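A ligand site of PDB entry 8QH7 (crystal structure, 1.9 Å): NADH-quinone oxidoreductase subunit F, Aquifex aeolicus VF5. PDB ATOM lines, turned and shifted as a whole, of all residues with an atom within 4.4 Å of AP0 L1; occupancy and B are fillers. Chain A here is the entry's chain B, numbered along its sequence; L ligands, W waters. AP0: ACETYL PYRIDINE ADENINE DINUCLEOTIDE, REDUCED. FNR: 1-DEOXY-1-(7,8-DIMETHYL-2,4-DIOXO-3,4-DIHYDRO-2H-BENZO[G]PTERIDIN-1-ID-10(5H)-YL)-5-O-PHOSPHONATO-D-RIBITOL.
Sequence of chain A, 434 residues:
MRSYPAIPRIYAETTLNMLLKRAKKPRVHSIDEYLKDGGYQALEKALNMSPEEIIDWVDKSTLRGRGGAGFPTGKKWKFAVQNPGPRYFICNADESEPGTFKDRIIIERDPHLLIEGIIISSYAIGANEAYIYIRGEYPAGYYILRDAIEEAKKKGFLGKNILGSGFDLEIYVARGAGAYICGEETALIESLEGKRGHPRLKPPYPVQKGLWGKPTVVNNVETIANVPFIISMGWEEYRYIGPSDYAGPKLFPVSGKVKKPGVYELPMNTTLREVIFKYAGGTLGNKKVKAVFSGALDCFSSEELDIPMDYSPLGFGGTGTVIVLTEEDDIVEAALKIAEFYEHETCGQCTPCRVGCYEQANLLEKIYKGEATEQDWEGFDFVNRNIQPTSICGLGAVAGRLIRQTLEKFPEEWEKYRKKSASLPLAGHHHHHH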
ATOM      1  N   GLY A  67       3.732 -17.433  -1.087  1.00  0.00           N
ATOM      2  CA  GLY A  67       2.960 -18.236  -2.026  1.00  0.00           C
ATOM      3  C   GLY A  67       3.603 -18.262  -3.408  1.00  0.00           C
ATOM      4  O   GLY A  67       3.167 -19.048  -4.240  1.00  0.00           O
ATOM      5  N   GLY A  68       4.567 -17.349  -3.668  1.00  0.00           N
ATOM      6  CA  GLY A  68       5.333 -17.382  -4.906  1.00  0.00           C
ATOM      7  C   GLY A  68       5.562 -16.009  -5.554  1.00  0.00           C
ATOM      8  O   GLY A  68       6.565 -15.843  -6.241  1.00  0.00           O
ATOM      9  N   ALA A  69       4.658 -15.046  -5.366  1.00  0.00           N
ATOM     10  CA  ALA A  69       4.758 -13.758  -6.038  1.00  0.00           C
ATOM     11  C   ALA A  69       5.588 -12.755  -5.233  1.00  0.00           C
ATOM     12  O   ALA A  69       6.072 -11.771  -5.798  1.00  0.00           O
ATOM     13  CB  ALA A  69       3.396 -13.187  -6.357  1.00  0.00           C
ATOM     14  N   PHE A  71       4.708 -10.532  -2.878  1.00  0.00           N
ATOM     15  CA  PHE A  71       4.113  -9.242  -2.582  1.00  0.00           C
ATOM     16  C   PHE A  71       4.332  -8.899  -1.110  1.00  0.00           C
ATOM     17  O   PHE A  71       4.127  -9.753  -0.236  1.00  0.00           O
ATOM     18  CB  PHE A  71       2.631  -9.192  -2.951  1.00  0.00           C
ATOM     19  CG  PHE A  71       2.042  -7.802  -2.952  1.00  0.00           C
ATOM     20  CD1 PHE A  71       2.081  -7.006  -4.094  1.00  0.00           C
ATOM     21  CD2 PHE A  71       1.470  -7.276  -1.813  1.00  0.00           C
ATOM     22  CE1 PHE A  71       1.553  -5.722  -4.085  1.00  0.00           C
ATOM     23  CE2 PHE A  71       0.952  -5.986  -1.796  1.00  0.00           C
ATOM     24  CZ  PHE A  71       0.986  -5.212  -2.940  1.00  0.00           C
ATOM     25  N   LYS A  76       0.014  -5.331   1.740  1.00  0.00           N
ATOM     26  CA  LYS A  76      -1.253  -5.954   1.376  1.00  0.00           C
ATOM     27  C   LYS A  76      -2.305  -5.660   2.445  1.00  0.00           C
ATOM     28  O   LYS A  76      -3.417  -5.264   2.115  1.00  0.00           O
ATOM     29  CB  LYS A  76      -1.109  -7.475   1.153  1.00  0.00           C
ATOM     30  CG  LYS A  76      -2.301  -8.127   0.474  1.00  0.00           C
ATOM     31  CD  LYS A  76      -2.252  -9.643   0.394  1.00  0.00           C
ATOM     32  CE  LYS A  76      -1.087 -10.190  -0.393  1.00  0.00           C
ATOM     33  NZ  LYS A  76      -1.232 -11.645  -0.596  1.00  0.00           N
ATOM     34  N   PHE A  79      -3.580  -2.035   2.417  1.00  0.00           N
ATOM     35  CA  PHE A  79      -4.554  -1.842   1.356  1.00  0.00           C
ATOM     36  C   PHE A  79      -5.937  -2.301   1.817  1.00  0.00           C
ATOM     37  O   PHE A  79      -6.923  -1.624   1.547  1.00  0.00           O
ATOM     38  CB  PHE A  79      -4.173  -2.552   0.059  1.00  0.00           C
ATOM     39  CG  PHE A  79      -3.189  -1.825  -0.820  1.00  0.00           C
ATOM     40  CD1 PHE A  79      -3.536  -0.621  -1.428  1.00  0.00           C
ATOM     41  CD2 PHE A  79      -1.927  -2.334  -1.066  1.00  0.00           C
ATOM     42  CE1 PHE A  79      -2.637   0.055  -2.234  1.00  0.00           C
ATOM     43  CE2 PHE A  79      -1.021  -1.664  -1.876  1.00  0.00           C
ATOM     44  CZ  PHE A  79      -1.373  -0.466  -2.461  1.00  0.00           C
ATOM     45  N   GLU A  95      -1.804 -25.399  -1.989  1.00  0.00           N
ATOM     46  CA  GLU A  95      -0.508 -25.881  -2.457  1.00  0.00           C
ATOM     47  C   GLU A  95      -0.606 -27.054  -3.453  1.00  0.00           C
ATOM     48  O   GLU A  95      -0.725 -28.208  -3.049  1.00  0.00           O
ATOM     49  CB  GLU A  95       0.335 -26.304  -1.244  1.00  0.00           C
ATOM     50  CG  GLU A  95       1.702 -26.873  -1.615  1.00  0.00           C
ATOM     51  CD  GLU A  95       2.589 -27.118  -0.413  1.00  0.00           C
ATOM     52  OE1 GLU A  95       2.232 -28.006   0.400  1.00  0.00           O
ATOM     53  OE2 GLU A  95       3.603 -26.380  -0.271  1.00  0.00           O
ATOM     54  N   SER A  96      -0.512 -26.736  -4.749  1.00  0.00           N
ATOM     55  CA  SER A  96      -0.653 -27.735  -5.796  1.00  0.00           C
ATOM     56  C   SER A  96       0.371 -27.578  -6.916  1.00  0.00           C
ATOM     57  O   SER A  96       0.307 -28.333  -7.888  1.00  0.00           O
ATOM     58  CB  SER A  96      -2.061 -27.709  -6.369  1.00  0.00           C
ATOM     59  OG  SER A  96      -2.994 -28.173  -5.411  1.00  0.00           O
ATOM     60  N   GLU A  97       1.294 -26.611  -6.793  1.00  0.00           N
ATOM     61  CA  GLU A  97       2.380 -26.438  -7.761  1.00  0.00           C
ATOM     62  C   GLU A  97       3.256 -27.679  -7.774  1.00  0.00           C
ATOM     63  O   GLU A  97       3.665 -28.155  -6.710  1.00  0.00           O
ATOM     64  CB  GLU A  97       3.234 -25.219  -7.384  1.00  0.00           C
ATOM     65  CG  GLU A  97       4.310 -24.856  -8.392  1.00  0.00           C
ATOM     66  CD  GLU A  97       3.813 -24.170  -9.657  1.00  0.00           C
ATOM     67  OE1 GLU A  97       2.593 -24.209  -9.916  1.00  0.00           O
ATOM     68  OE2 GLU A  97       4.661 -23.581 -10.378  1.00  0.00           O
ATOM     69  N   THR A 100       6.067 -28.823  -5.042  1.00  0.00           N
ATOM     70  CA  THR A 100       5.854 -27.936  -3.901  1.00  0.00           C
ATOM     71  C   THR A 100       5.121 -28.673  -2.781  1.00  0.00           C
ATOM     72  O   THR A 100       3.961 -29.079  -2.932  1.00  0.00           O
ATOM     73  CB  THR A 100       5.151 -26.656  -4.347  1.00  0.00           C
ATOM     74  OG1 THR A 100       5.774 -26.187  -5.543  1.00  0.00           O
ATOM     75  CG2 THR A 100       5.196 -25.582  -3.277  1.00  0.00           C
ATOM     76  N   TYR A 180      -6.231 -27.136  -9.403  1.00  0.00           N
ATOM     77  CA  TYR A 180      -5.057 -26.292  -9.192  1.00  0.00           C
ATOM     78  C   TYR A 180      -5.423 -24.818  -9.200  1.00  0.00           C
ATOM     79  O   TYR A 180      -4.828 -24.018  -8.481  1.00  0.00           O
ATOM     80  CB  TYR A 180      -4.056 -26.603 -10.296  1.00  0.00           C
ATOM     81  CG  TYR A 180      -2.867 -25.698 -10.504  1.00  0.00           C
ATOM     82  CD1 TYR A 180      -1.771 -25.713  -9.655  1.00  0.00           C
ATOM     83  CD2 TYR A 180      -2.786 -24.906 -11.643  1.00  0.00           C
ATOM     84  CE1 TYR A 180      -0.651 -24.927  -9.908  1.00  0.00           C
ATOM     85  CE2 TYR A 180      -1.687 -24.119 -11.909  1.00  0.00           C
ATOM     86  CZ  TYR A 180      -0.600 -24.138 -11.045  1.00  0.00           C
ATOM     87  OH  TYR A 180       0.509 -23.394 -11.378  1.00  0.00           O
ATOM     88  N   GLU A 185      -6.046 -16.714  -6.040  1.00  0.00           N
ATOM     89  CA  GLU A 185      -6.763 -16.166  -4.888  1.00  0.00           C
ATOM     90  C   GLU A 185      -8.232 -15.869  -5.220  1.00  0.00           C
ATOM     91  O   GLU A 185      -9.074 -15.989  -4.352  1.00  0.00           O
ATOM     92  CB  GLU A 185      -6.055 -14.927  -4.354  1.00  0.00           C
ATOM     93  CG  GLU A 185      -5.893 -13.830  -5.398  1.00  0.00           C
ATOM     94  CD  GLU A 185      -5.197 -12.593  -4.858  1.00  0.00           C
ATOM     95  OE1 GLU A 185      -4.835 -12.598  -3.645  1.00  0.00           O
ATOM     96  OE2 GLU A 185      -5.008 -11.627  -5.649  1.00  0.00           O
ATOM     97  N   TYR A 205      -8.357  -6.084  -6.694  1.00  0.00           N
ATOM     98  CA  TYR A 205      -7.670  -7.081  -5.880  1.00  0.00           C
ATOM     99  C   TYR A 205      -8.583  -7.478  -4.719  1.00  0.00           C
ATOM    100  O   TYR A 205      -9.481  -6.715  -4.336  1.00  0.00           O
ATOM    101  CB  TYR A 205      -6.287  -6.561  -5.465  1.00  0.00           C
ATOM    102  CG  TYR A 205      -5.346  -6.450  -6.634  1.00  0.00           C
ATOM    103  CD1 TYR A 205      -4.721  -7.583  -7.149  1.00  0.00           C
ATOM    104  CD2 TYR A 205      -5.166  -5.257  -7.303  1.00  0.00           C
ATOM    105  CE1 TYR A 205      -3.897  -7.500  -8.259  1.00  0.00           C
ATOM    106  CE2 TYR A 205      -4.347  -5.160  -8.420  1.00  0.00           C
ATOM    107  CZ  TYR A 205      -3.707  -6.285  -8.896  1.00  0.00           C
ATOM    108  OH  TYR A 205      -2.915  -6.178  -9.998  1.00  0.00           O
ATOM    109  N   PRO A 206      -8.414  -8.691  -4.132  1.00  0.00           N
ATOM    110  CA  PRO A 206      -9.262  -9.131  -3.019  1.00  0.00           C
ATOM    111  C   PRO A 206      -9.372  -8.120  -1.880  1.00  0.00           C
ATOM    112  O   PRO A 206     -10.421  -8.012  -1.267  1.00  0.00           O
ATOM    113  CB  PRO A 206      -8.611 -10.436  -2.576  1.00  0.00           C
ATOM    114  CG  PRO A 206      -8.026 -10.981  -3.858  1.00  0.00           C
ATOM    115  CD  PRO A 206      -7.492  -9.754  -4.557  1.00  0.00           C
ATOM    116  N   VAL A 207      -8.286  -7.356  -1.632  1.00  0.00           N
ATOM    117  CA  VAL A 207      -8.231  -6.431  -0.505  1.00  0.00           C
ATOM    118  C   VAL A 207      -9.210  -5.271  -0.693  1.00  0.00           C
ATOM    119  O   VAL A 207      -9.575  -4.622   0.286  1.00  0.00           O
ATOM    120  CB  VAL A 207      -6.793  -5.921  -0.294  1.00  0.00           C
ATOM    121  CG1 VAL A 207      -5.887  -7.026   0.224  1.00  0.00           C
ATOM    122  CG2 VAL A 207      -6.220  -5.259  -1.533  1.00  0.00           C
ATOM    123  N   VAL A 218      -5.822 -12.532   1.185  1.00  0.00           N
ATOM    124  CA  VAL A 218      -5.375 -13.898   0.987  1.00  0.00           C
ATOM    125  C   VAL A 218      -3.870 -13.924   1.217  1.00  0.00           C
ATOM    126  O   VAL A 218      -3.130 -13.136   0.613  1.00  0.00           O
ATOM    127  CB  VAL A 218      -5.758 -14.421  -0.411  1.00  0.00           C
ATOM    128  CG1 VAL A 218      -5.346 -15.872  -0.598  1.00  0.00           C
ATOM    129  CG2 VAL A 218      -7.249 -14.235  -0.674  1.00  0.00           C
ATOM    130  N   LEU A 297       7.124 -22.977 -13.142  1.00  0.00           N
ATOM    131  CA  LEU A 297       7.237 -21.557 -13.474  1.00  0.00           C
ATOM    132  C   LEU A 297       8.508 -21.244 -14.278  1.00  0.00           C
ATOM    133  O   LEU A 297       8.401 -20.557 -15.297  1.00  0.00           O
ATOM    134  CB  LEU A 297       7.183 -20.749 -12.174  1.00  0.00           C
ATOM    135  CG  LEU A 297       7.275 -19.234 -12.313  1.00  0.00           C
ATOM    136  CD1 LEU A 297       6.035 -18.674 -13.012  1.00  0.00           C
ATOM    137  CD2 LEU A 297       7.465 -18.596 -10.942  1.00  0.00           C
ATOM    138  N   GLY A 318       9.904 -17.254  -6.980  1.00  0.00           N
ATOM    139  CA  GLY A 318       8.862 -18.263  -6.980  1.00  0.00           C
ATOM    140  C   GLY A 318       8.550 -18.766  -5.574  1.00  0.00           C
ATOM    141  O   GLY A 318       8.621 -18.016  -4.607  1.00  0.00           O
ATOM    142  N   THR A 319       8.219 -20.050  -5.486  1.00  0.00           N
ATOM    143  CA  THR A 319       7.852 -20.713  -4.240  1.00  0.00           C
ATOM    144  C   THR A 319       9.099 -21.152  -3.456  1.00  0.00           C
ATOM    145  O   THR A 319       8.979 -21.536  -2.305  1.00  0.00           O
ATOM    146  CB  THR A 319       6.961 -21.933  -4.556  1.00  0.00           C
ATOM    147  OG1 THR A 319       7.662 -22.771  -5.474  1.00  0.00           O
ATOM    148  CG2 THR A 319       5.621 -21.572  -5.145  1.00  0.00           C
HETATM  149  O7N AP0 L   1       0.907 -24.224  -5.064  1.00  0.00           O
HETATM  150  C7N AP0 L   1       1.372 -23.101  -5.062  1.00  0.00           C
HETATM  151  C8N AP0 L   1       2.089 -22.602  -3.841  1.00  0.00           C
HETATM  152  C3N AP0 L   1       1.252 -22.246  -6.267  1.00  0.00           C
HETATM  153  C4N AP0 L   1       0.493 -22.795  -7.445  1.00  0.00           C
HETATM  154  C5N AP0 L   1       0.475 -21.840  -8.567  1.00  0.00           C
HETATM  155  C6N AP0 L   1       1.079 -20.663  -8.529  1.00  0.00           C
HETATM  156  C2N AP0 L   1       1.850 -21.042  -6.322  1.00  0.00           C
HETATM  157  N1N AP0 L   1       1.766 -20.225  -7.439  1.00  0.00           N
HETATM  158  C1D AP0 L   1       2.426 -18.913  -7.470  1.00  0.00           C
HETATM  159  C2D AP0 L   1       3.531 -18.778  -8.519  1.00  0.00           C
HETATM  160  O2D AP0 L   1       4.818 -19.030  -7.954  1.00  0.00           O
HETATM  161  C3D AP0 L   1       3.391 -17.308  -9.007  1.00  0.00           C
HETATM  162  O3D AP0 L   1       4.557 -16.547  -8.718  1.00  0.00           O
HETATM  163  O4D AP0 L   1       1.453 -17.925  -7.768  1.00  0.00           O
HETATM  164  C4D AP0 L   1       2.193 -16.760  -8.205  1.00  0.00           C
HETATM  165  C5D AP0 L   1       1.296 -15.812  -8.967  1.00  0.00           C
HETATM  166  O5D AP0 L   1       0.280 -15.344  -8.061  1.00  0.00           O
HETATM  167  PN  AP0 L   1      -0.635 -14.091  -8.394  1.00  0.00           P
HETATM  168  O1N AP0 L   1      -1.110 -14.194  -9.787  1.00  0.00           O
HETATM  169  O2N AP0 L   1      -1.610 -13.947  -7.275  1.00  0.00           O
HETATM  170  O3  AP0 L   1       0.442 -12.915  -8.280  1.00  0.00           O
HETATM  171  PA  AP0 L   1       0.416 -11.325  -8.265  1.00  0.00           P
HETATM  172  O1A AP0 L   1      -0.526 -10.838  -9.299  1.00  0.00           O
HETATM  173  O2A AP0 L   1       1.837 -10.906  -8.318  1.00  0.00           O
HETATM  174  O5B AP0 L   1      -0.200 -10.973  -6.837  1.00  0.00           O
HETATM  175  C5B AP0 L   1       0.474 -11.369  -5.611  1.00  0.00           C
HETATM  176  C4B AP0 L   1      -0.334 -10.934  -4.405  1.00  0.00           C
HETATM  177  O4B AP0 L   1      -0.212  -9.504  -4.229  1.00  0.00           O
HETATM  178  C1B AP0 L   1      -1.492  -8.888  -4.355  1.00  0.00           C
HETATM  179  C2B AP0 L   1      -2.396  -9.917  -5.031  1.00  0.00           C
HETATM  180  O2B AP0 L   1      -3.751  -9.672  -4.668  1.00  0.00           O
HETATM  181  C3B AP0 L   1      -1.827 -11.230  -4.476  1.00  0.00           C
HETATM  182  O3B AP0 L   1      -2.380 -11.561  -3.187  1.00  0.00           O
HETATM  183  N9A AP0 L   1      -1.351  -7.670  -5.124  1.00  0.00           N
HETATM  184  C8A AP0 L   1      -0.637  -7.491  -6.291  1.00  0.00           C
HETATM  185  N7A AP0 L   1      -0.732  -6.295  -6.802  1.00  0.00           N
HETATM  186  C5A AP0 L   1      -1.575  -5.621  -5.916  1.00  0.00           C
HETATM  187  C6A AP0 L   1      -2.082  -4.301  -5.898  1.00  0.00           C
HETATM  188  N6A AP0 L   1      -1.830  -3.396  -6.861  1.00  0.00           N
HETATM  189  C4A AP0 L   1      -1.956  -6.457  -4.882  1.00  0.00           C
HETATM  190  N3A AP0 L   1      -2.747  -6.136  -3.848  1.00  0.00           N
HETATM  191  C2A AP0 L   1      -3.162  -4.862  -3.924  1.00  0.00           C
HETATM  192  N1A AP0 L   1      -2.880  -3.951  -4.867  1.00  0.00           N
HETATM  193  C9A FNR L   2      -1.658 -19.187  -7.161  1.00  0.00           C
HETATM  194  N10 FNR L   2      -1.249 -18.739  -5.877  1.00  0.00           N
HETATM  195  CAA FNR L   2      -1.240 -19.649  -4.832  1.00  0.00           C
HETATM  196  N1  FNR L   2      -0.900 -19.206  -3.585  1.00  0.00           N
HETATM  197  C2  FNR L   2      -0.885 -20.037  -2.495  1.00  0.00           C
HETATM  198  O2  FNR L   2      -0.685 -19.609  -1.365  1.00  0.00           O
HETATM  199  N3  FNR L   2      -1.180 -21.350  -2.739  1.00  0.00           N
HETATM  200  C4  FNR L   2      -1.569 -21.901  -3.940  1.00  0.00           C
HETATM  201  O4  FNR L   2      -1.837 -23.107  -4.022  1.00  0.00           O
HETATM  202  C4A FNR L   2      -1.608 -20.959  -5.010  1.00  0.00           C
HETATM  203  N5  FNR L   2      -2.023 -21.380  -6.220  1.00  0.00           N
HETATM  204  C5A FNR L   2      -2.073 -20.522  -7.311  1.00  0.00           C
HETATM  205  C6  FNR L   2      -2.471 -20.998  -8.560  1.00  0.00           C
HETATM  206  C7  FNR L   2      -2.470 -20.154  -9.666  1.00  0.00           C
HETATM  207  C7M FNR L   2      -2.925 -20.690 -11.000  1.00  0.00           C
HETATM  208  C8  FNR L   2      -2.055 -18.820  -9.516  1.00  0.00           C
HETATM  209  C8M FNR L   2      -2.010 -17.897 -10.705  1.00  0.00           C
HETATM  210  C9  FNR L   2      -1.661 -18.342  -8.276  1.00  0.00           C
HETATM  211  C1' FNR L   2      -0.920 -17.328  -5.642  1.00  0.00           C
HETATM  212  C2' FNR L   2      -2.155 -16.659  -5.046  1.00  0.00           C
HETATM  213  O2' FNR L   2      -2.992 -16.206  -6.122  1.00  0.00           O
HETATM  214  C3' FNR L   2      -1.744 -15.482  -4.156  1.00  0.00           C
HETATM  215  O3' FNR L   2      -0.748 -14.703  -4.798  1.00  0.00           O
HETATM  216  C4' FNR L   2      -1.203 -15.870  -2.780  1.00  0.00           C
HETATM  217  O4' FNR L   2      -2.014 -16.880  -2.173  1.00  0.00           O
HETATM  218  C5' FNR L   2      -1.095 -14.658  -1.892  1.00  0.00           C
HETATM  219  O5' FNR L   2      -0.450 -15.017  -0.646  1.00  0.00           O
HETATM  220  P   FNR L   2       1.045 -14.469  -0.321  1.00  0.00           P
HETATM  221  O1P FNR L   2       1.090 -12.981  -0.621  1.00  0.00           O
HETATM  222  O2P FNR L   2       1.219 -14.769   1.158  1.00  0.00           O
HETATM  223  O3P FNR L   2       1.981 -15.251  -1.213  1.00  0.00           O
HETATM  224  O   HOH W   1       3.274 -23.691  -1.246  1.00  0.00           O
HETATM  225  O   HOH W   2      -4.677  -8.333  -2.571  1.00  0.00           O
HETATM  226  O   HOH W   3       0.485 -13.664 -11.841  1.00  0.00           O
HETATM  227  O   HOH W   4       1.015  -6.121  -9.133  1.00  0.00           O
HETATM  228  O   HOH W   5      -4.319  -1.561  -5.074  1.00  0.00           O
HETATM  229  O   HOH W   6       4.853 -14.502 -10.287  1.00  0.00           O
HETATM  230  O   HOH W   7       3.928 -12.127  -9.828  1.00  0.00           O
HETATM  231  O   HOH W   8       5.705 -21.424  -8.954  1.00  0.00           O
HETATM  232  O   HOH W   9      -3.022 -10.676  -9.748  1.00  0.00           O
HETATM  233  O   HOH W  10       1.979 -19.564 -11.604  1.00  0.00           O
HETATM  234  O   HOH W  11      -4.012 -12.482  -8.091  1.00  0.00           O
HETATM  235  O   HOH W  12      -3.524 -14.504 -11.023  1.00  0.00           O
HETATM  236  O   HOH W  13       2.966  -8.251  -7.399  1.00  0.00           O
HETATM  237  O   HOH W  14      -0.121  -8.143 -10.202  1.00  0.00           O
HETATM  238  O   HOH W  15      -0.574  -3.973  -9.349  1.00  0.00           O
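NZ of Lys 76 lies within hydrogen-bond range of O3B of AP0 L1, at 2.8 Å. N of Glu 97 lies within hydrogen-bond range of O7N of AP0 L1 (3.0 Å). N of Gly 67 sits at hydrogen-bond distance from O3P of FNR L2 (2.8 Å). N of Ser 96 sits at hydrogen-bond distance from O7N of AP0 L1, at 2.9 Å. The backbone carbonyl oxygen of Gly 68 sits at hydrogen-bond distance from an oxygen (O3D) of AP0 L1 (3.3 Å). N of Glu 185 sits at hydrogen-bond distance from O2' of FNR L2, at 3.1 Å. An oxygen (O4) of FNR L2 is in hydrogen-bond range of the backbone NH (N) of Glu 95, 3.1 Å away. An oxygen (O1P) of FNR L2 lies within salt-bridge range of the side-chain amino group of Lys 76. O2B of AP0 L1 is in hydrogen-bond range of OE2 of Glu 185 (2.5 Å).
An oxygen (O2N) of AP0 L1 is in hydrogen-bond range of an oxygen (O3') of FNR L2 (2.7 Å).
The side-chain carboxylate (OE1) of Glu 97 sits at hydrogen-bond distance from the side-chain hydroxyl (OH) of Tyr 180, 2.7 Å away. NZ of Lys 76 lies within hydrogen-bond range of O of Val 218 (2.7 Å). OG1 of Thr 100 sits at hydrogen-bond distance from O of Glu 97 (3.1 Å).
Gly 67 touches AP0 L1. Ala 69 touches AP0 L1 (CB to O2A, 3.4 Å). Phe 71 touches AP0 L1 (CG to O4B, 3.1 Å). CA of Glu 95 touches O7N of AP0 L1, at 3.4 Å. OH of Tyr 180 touches C5N of AP0 L1, 3.2 Å away. CD1 of Tyr 205 touches O2B of AP0 L1, 3.4 Å away. Pro 206 touches AP0 L1 (CD to O2B, 3.7 Å). Val 207 touches AP0 L1. Thr 319 touches AP0 L1 (CG2 to O2D, 3.9 Å). Along chain A the residues within 4 Å of AP0 L1 span positions 67 to 319. The nearest printed residue that does not touch AP0 L1 is Phe 79 (4.01 Å).
Water W8 bridges an oxygen (O2D) of AP0 L1 and the side-chain carboxylate (OE2) of Glu 97. Water W15 bridges a nitrogen (N6A) of AP0 L1 (2.8 Å) and the side-chain hydroxyl (OH) of Tyr 205 (3.3 Å). Water W14 lies within hydrogen-bond range of O1A of AP0 L1 (2.9 Å) and OH of Tyr 205 (3.4 Å). Water W11 lies within hydrogen-bond range of the side-chain carboxylate (OE2) of Glu 185 and an oxygen (O2N) of AP0 L1.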
